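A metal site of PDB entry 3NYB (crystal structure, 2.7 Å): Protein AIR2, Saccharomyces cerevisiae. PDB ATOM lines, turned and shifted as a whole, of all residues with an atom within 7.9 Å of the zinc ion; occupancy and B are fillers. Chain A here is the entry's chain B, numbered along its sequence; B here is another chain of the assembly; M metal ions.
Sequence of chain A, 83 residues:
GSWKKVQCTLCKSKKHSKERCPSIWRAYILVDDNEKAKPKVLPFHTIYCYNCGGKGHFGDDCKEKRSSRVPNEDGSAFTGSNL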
ATOM      1  N   TYR A  48      -3.698  26.728 -16.423  1.00  0.00           N
ATOM      2  CA  TYR A  48      -2.836  25.798 -17.128  1.00  0.00           C
ATOM      3  C   TYR A  48      -3.402  25.400 -18.475  1.00  0.00           C
ATOM      4  O   TYR A  48      -4.590  25.141 -18.610  1.00  0.00           O
ATOM      5  CB  TYR A  48      -2.558  24.566 -16.270  1.00  0.00           C
ATOM      6  CG  TYR A  48      -1.733  24.880 -15.048  1.00  0.00           C
ATOM      7  CD1 TYR A  48      -2.349  25.215 -13.851  1.00  0.00           C
ATOM      8  CD2 TYR A  48      -0.353  24.836 -15.089  1.00  0.00           C
ATOM      9  CE1 TYR A  48      -1.594  25.500 -12.723  1.00  0.00           C
ATOM     10  CE2 TYR A  48       0.409  25.112 -13.969  1.00  0.00           C
ATOM     11  CZ  TYR A  48      -0.227  25.450 -12.783  1.00  0.00           C
ATOM     12  OH  TYR A  48       0.525  25.733 -11.668  1.00  0.00           O
ATOM     13  N   CYS A  49      -2.534  25.351 -19.476  1.00  0.00           N
ATOM     14  CA  CYS A  49      -2.958  25.083 -20.837  1.00  0.00           C
ATOM     15  C   CYS A  49      -2.816  23.603 -21.186  1.00  0.00           C
ATOM     16  O   CYS A  49      -1.778  22.993 -20.955  1.00  0.00           O
ATOM     17  CB  CYS A  49      -2.139  25.918 -21.813  1.00  0.00           C
ATOM     18  SG  CYS A  49      -2.266  25.335 -23.497  1.00  0.00           S
ATOM     19  N   TYR A  50      -3.874  23.035 -21.755  1.00  0.00           N
ATOM     20  CA  TYR A  50      -3.899  21.612 -22.045  1.00  0.00           C
ATOM     21  C   TYR A  50      -3.113  21.284 -23.299  1.00  0.00           C
ATOM     22  O   TYR A  50      -2.818  20.123 -23.573  1.00  0.00           O
ATOM     23  CB  TYR A  50      -5.340  21.113 -22.159  1.00  0.00           C
ATOM     24  CG  TYR A  50      -6.157  21.673 -23.303  1.00  0.00           C
ATOM     25  CD1 TYR A  50      -5.768  21.494 -24.628  1.00  0.00           C
ATOM     26  CD2 TYR A  50      -7.342  22.352 -23.057  1.00  0.00           C
ATOM     27  CE1 TYR A  50      -6.538  21.994 -25.670  1.00  0.00           C
ATOM     28  CE2 TYR A  50      -8.113  22.853 -24.098  1.00  0.00           C
ATOM     29  CZ  TYR A  50      -7.714  22.669 -25.396  1.00  0.00           C
ATOM     30  OH  TYR A  50      -8.485  23.172 -26.415  1.00  0.00           O
ATOM     31  N   ASN A  51      -2.754  22.319 -24.039  1.00  0.00           N
ATOM     32  CA  ASN A  51      -2.055  22.184 -25.312  1.00  0.00           C
ATOM     33  C   ASN A  51      -0.538  22.191 -25.134  1.00  0.00           C
ATOM     34  O   ASN A  51       0.168  21.342 -25.682  1.00  0.00           O
ATOM     35  CB  ASN A  51      -2.472  23.297 -26.257  1.00  0.00           C
ATOM     36  CG  ASN A  51      -1.936  23.105 -27.652  1.00  0.00           C
ATOM     37  OD1 ASN A  51      -1.506  24.055 -28.300  1.00  0.00           O
ATOM     38  ND2 ASN A  51      -1.943  21.866 -28.110  1.00  0.00           N
ATOM     39  N   CYS A  52      -0.041  23.166 -24.377  1.00  0.00           N
ATOM     40  CA  CYS A  52       1.334  23.190 -23.922  1.00  0.00           C
ATOM     41  C   CYS A  52       1.263  23.244 -22.410  1.00  0.00           C
ATOM     42  O   CYS A  52       0.388  23.905 -21.852  1.00  0.00           O
ATOM     43  CB  CYS A  52       2.052  24.436 -24.447  1.00  0.00           C
ATOM     44  SG  CYS A  52       1.702  25.905 -23.461  1.00  0.00           S
ATOM     45  N   GLY A  53       2.162  22.547 -21.734  1.00  0.00           N
ATOM     46  CA  GLY A  53       2.103  22.483 -20.284  1.00  0.00           C
ATOM     47  C   GLY A  53       2.322  23.822 -19.623  1.00  0.00           C
ATOM     48  O   GLY A  53       2.646  23.898 -18.444  1.00  0.00           O
ATOM     49  N   GLY A  54       2.125  24.898 -20.384  1.00  0.00           N
ATOM     50  CA  GLY A  54       2.394  26.249 -19.911  1.00  0.00           C
ATOM     51  C   GLY A  54       1.303  26.858 -19.050  1.00  0.00           C
ATOM     52  O   GLY A  54       0.118  26.536 -19.196  1.00  0.00           O
ATOM     53  N   LYS A  55       1.704  27.753 -18.154  1.00  0.00           N
ATOM     54  CA  LYS A  55       0.780  28.411 -17.238  1.00  0.00           C
ATOM     55  C   LYS A  55       0.396  29.806 -17.708  1.00  0.00           C
ATOM     56  O   LYS A  55       1.125  30.412 -18.488  1.00  0.00           O
ATOM     57  CB  LYS A  55       1.382  28.492 -15.833  1.00  0.00           C
ATOM     58  CG  LYS A  55       2.666  29.276 -15.773  1.00  0.00           C
ATOM     59  CD  LYS A  55       3.655  28.682 -14.776  1.00  0.00           C
ATOM     60  CE  LYS A  55       3.051  28.552 -13.390  1.00  0.00           C
ATOM     61  NZ  LYS A  55       4.046  28.006 -12.434  1.00  0.00           N
ATOM     62  N   HIS A  57      -2.631  30.636 -19.222  1.00  0.00           N
ATOM     63  CA  HIS A  57      -3.666  30.644 -20.244  1.00  0.00           C
ATOM     64  C   HIS A  57      -4.270  29.257 -20.465  1.00  0.00           C
ATOM     65  O   HIS A  57      -3.632  28.243 -20.147  1.00  0.00           O
ATOM     66  CB  HIS A  57      -3.099  31.165 -21.574  1.00  0.00           C
ATOM     67  CG  HIS A  57      -2.098  30.249 -22.194  1.00  0.00           C
ATOM     68  ND1 HIS A  57      -0.781  30.181 -21.772  1.00  0.00           N
ATOM     69  CD2 HIS A  57      -2.211  29.373 -23.221  1.00  0.00           C
ATOM     70  CE1 HIS A  57      -0.142  29.294 -22.503  1.00  0.00           C
ATOM     71  NE2 HIS A  57      -0.978  28.778 -23.384  1.00  0.00           N
ATOM     72  N   PHE A  58      -5.483  29.215 -20.993  1.00  0.00           N
ATOM     73  CA  PHE A  58      -6.154  27.950 -21.270  1.00  0.00           C
ATOM     74  C   PHE A  58      -5.681  27.278 -22.548  1.00  0.00           C
ATOM     75  O   PHE A  58      -5.319  27.954 -23.520  1.00  0.00           O
ATOM     76  CB  PHE A  58      -7.667  28.154 -21.340  1.00  0.00           C
ATOM     77  CG  PHE A  58      -8.287  28.500 -20.033  1.00  0.00           C
ATOM     78  CD1 PHE A  58      -8.139  27.670 -18.930  1.00  0.00           C
ATOM     79  CD2 PHE A  58      -9.040  29.654 -19.888  1.00  0.00           C
ATOM     80  CE1 PHE A  58      -8.710  27.986 -17.721  1.00  0.00           C
ATOM     81  CE2 PHE A  58      -9.622  29.977 -18.684  1.00  0.00           C
ATOM     82  CZ  PHE A  58      -9.451  29.130 -17.593  1.00  0.00           C
ATOM     83  N   GLY A  59      -5.689  25.955 -22.555  1.00  0.00           N
ATOM     84  CA  GLY A  59      -5.260  25.182 -23.712  1.00  0.00           C
ATOM     85  C   GLY A  59      -6.030  25.480 -24.984  1.00  0.00           C
ATOM     86  O   GLY A  59      -5.580  25.176 -26.087  1.00  0.00           O
ATOM     87  N   ASP A  60      -7.193  26.092 -24.828  1.00  0.00           N
ATOM     88  CA  ASP A  60      -8.060  26.327 -25.971  1.00  0.00           C
ATOM     89  C   ASP A  60      -7.606  27.533 -26.794  1.00  0.00           C
ATOM     90  O   ASP A  60      -7.577  27.469 -28.024  1.00  0.00           O
ATOM     91  CB  ASP A  60      -9.497  26.522 -25.493  1.00  0.00           C
ATOM     92  CG  ASP A  60     -10.503  25.934 -26.432  1.00  0.00           C
ATOM     93  OD1 ASP A  60     -10.852  26.590 -27.429  1.00  0.00           O
ATOM     94  OD2 ASP A  60     -10.947  24.800 -26.179  1.00  0.00           O
ATOM     95  N   ASP A  61      -7.259  28.627 -26.115  1.00  0.00           N
ATOM     96  CA  ASP A  61      -6.810  29.827 -26.793  1.00  0.00           C
ATOM     97  C   ASP A  61      -5.302  30.013 -26.661  1.00  0.00           C
ATOM     98  O   ASP A  61      -4.807  31.061 -26.255  1.00  0.00           O
ATOM     99  CB  ASP A  61      -7.578  31.059 -26.293  1.00  0.00           C
ATOM    100  CG  ASP A  61      -7.872  31.011 -24.809  1.00  0.00           C
ATOM    101  OD1 ASP A  61      -9.055  31.196 -24.446  1.00  0.00           O
ATOM    102  OD2 ASP A  61      -6.943  30.783 -24.007  1.00  0.00           O
ATOM    103  N   CYS A  62      -4.576  28.954 -27.011  1.00  0.00           N
ATOM    104  CA  CYS A  62      -3.130  28.914 -26.893  1.00  0.00           C
ATOM    105  C   CYS A  62      -2.478  29.195 -28.239  1.00  0.00           C
ATOM    106  O   CYS A  62      -3.128  29.072 -29.286  1.00  0.00           O
ATOM    107  CB  CYS A  62      -2.723  27.550 -26.308  1.00  0.00           C
ATOM    108  SG  CYS A  62      -1.120  26.892 -26.753  1.00  0.00           S
ATOM    109  N   LYS A  63      -1.207  29.587 -28.228  1.00  0.00           N
ATOM    110  CA  LYS A  63      -0.548  30.072 -29.443  1.00  0.00           C
ATOM    111  C   LYS A  63       0.147  28.990 -30.273  1.00  0.00           C
ATOM    112  O   LYS A  63       0.289  29.135 -31.485  1.00  0.00           O
ATOM    113  CB  LYS A  63       0.459  31.182 -29.105  1.00  0.00           C
ATOM    114  CG  LYS A  63      -0.142  32.308 -28.281  1.00  0.00           C
ATOM    115  CD  LYS A  63      -1.479  32.750 -28.843  1.00  0.00           C
ATOM    116  CE  LYS A  63      -2.175  33.739 -27.913  1.00  0.00           C
ATOM    117  NZ  LYS A  63      -3.611  33.930 -28.272  1.00  0.00           N
ATOM    118  N   GLU A  64       0.592  27.925 -29.607  1.00  0.00           N
ATOM    119  CA  GLU A  64       1.344  26.867 -30.270  1.00  0.00           C
ATOM    120  C   GLU A  64       0.490  26.028 -31.212  1.00  0.00           C
ATOM    121  O   GLU A  64      -0.737  26.053 -31.136  1.00  0.00           O
ATOM    122  CB  GLU A  64       1.979  25.959 -29.217  1.00  0.00           C
ATOM    123  CG  GLU A  64       2.717  26.704 -28.112  1.00  0.00           C
ATOM    124  CD  GLU A  64       4.127  27.094 -28.514  1.00  0.00           C
ATOM    125  OE1 GLU A  64       4.889  26.201 -28.943  1.00  0.00           O
ATOM    126  OE2 GLU A  64       4.476  28.290 -28.386  1.00  0.00           O
ATOM    127  N   LYS A  65       1.139  25.289 -32.117  1.00  0.00           N
ATOM    128  CA  LYS A  65       0.436  24.307 -32.925  1.00  0.00           C
ATOM    129  C   LYS A  65      -0.212  23.327 -31.963  1.00  0.00           C
ATOM    130  O   LYS A  65       0.398  22.947 -30.958  1.00  0.00           O
ATOM    131  CB  LYS A  65       1.403  23.555 -33.843  1.00  0.00           C
ATOM    132  CG  LYS A  65       1.877  24.325 -35.059  1.00  0.00           C
ATOM    133  CD  LYS A  65       2.405  23.381 -36.122  1.00  0.00           C
ATOM    134  CE  LYS A  65       3.114  24.130 -37.237  1.00  0.00           C
ATOM    135  NZ  LYS A  65       4.400  24.732 -36.785  1.00  0.00           N
ATOM    136  N   VAL B 234       1.761  17.411 -22.734  1.00  0.00           N
ATOM    137  CA  VAL B 234       1.372  17.862 -21.393  1.00  0.00           C
ATOM    138  C   VAL B 234       1.335  16.748 -20.348  1.00  0.00           C
ATOM    139  O   VAL B 234       0.833  15.663 -20.611  1.00  0.00           O
ATOM    140  CB  VAL B 234      -0.004  18.554 -21.416  1.00  0.00           C
ATOM    141  CG1 VAL B 234      -0.313  19.173 -20.063  1.00  0.00           C
ATOM    142  CG2 VAL B 234      -0.043  19.602 -22.502  1.00  0.00           C
HETATM  143 ZN    ZN M   1      -0.258  26.736 -24.480  1.00  0.00          ZN
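The zinc ion is bound by SG of Cys 52, at 2.4 Å. The zinc ion is bound by NE2 of His 57, 2.4 Å away. SG of Cys 62 binds the zinc ion, 2.4 Å away. The zinc ion is bound by SG of Cys 49 (2.6 Å).
The side-chain sulfur (SG) of Cys 62 sits close to the side-chain amide oxygen (OD1) of Asn 51, at 3.3 Å. The backbone NH of Gly 59 sits close to the side-chain sulfur of Cys 49, at 3.6 Å. The backbone NH of Cys 49 lies within hydrogen-bond range of the backbone carbonyl oxygen of Gly 54 (2.9 Å). The side-chain sulfur (SG) of Cys 62 lies close to the backbone NH (N) of Glu 64. The side-chain sulfur (SG) of Cys 49 lies close to the backbone NH (N) of Asn 51, 3.1 Å away. The side-chain sulfur (SG) of Cys 52 lies close to the backbone NH (N) of Gly 54 (3.3 Å).
Within 4 Å of the zinc ion: Cys 49, Cys 52, His 57 and Cys 62. Along chain A the residues within 4 Å of the zinc ion span positions 49 to 62.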
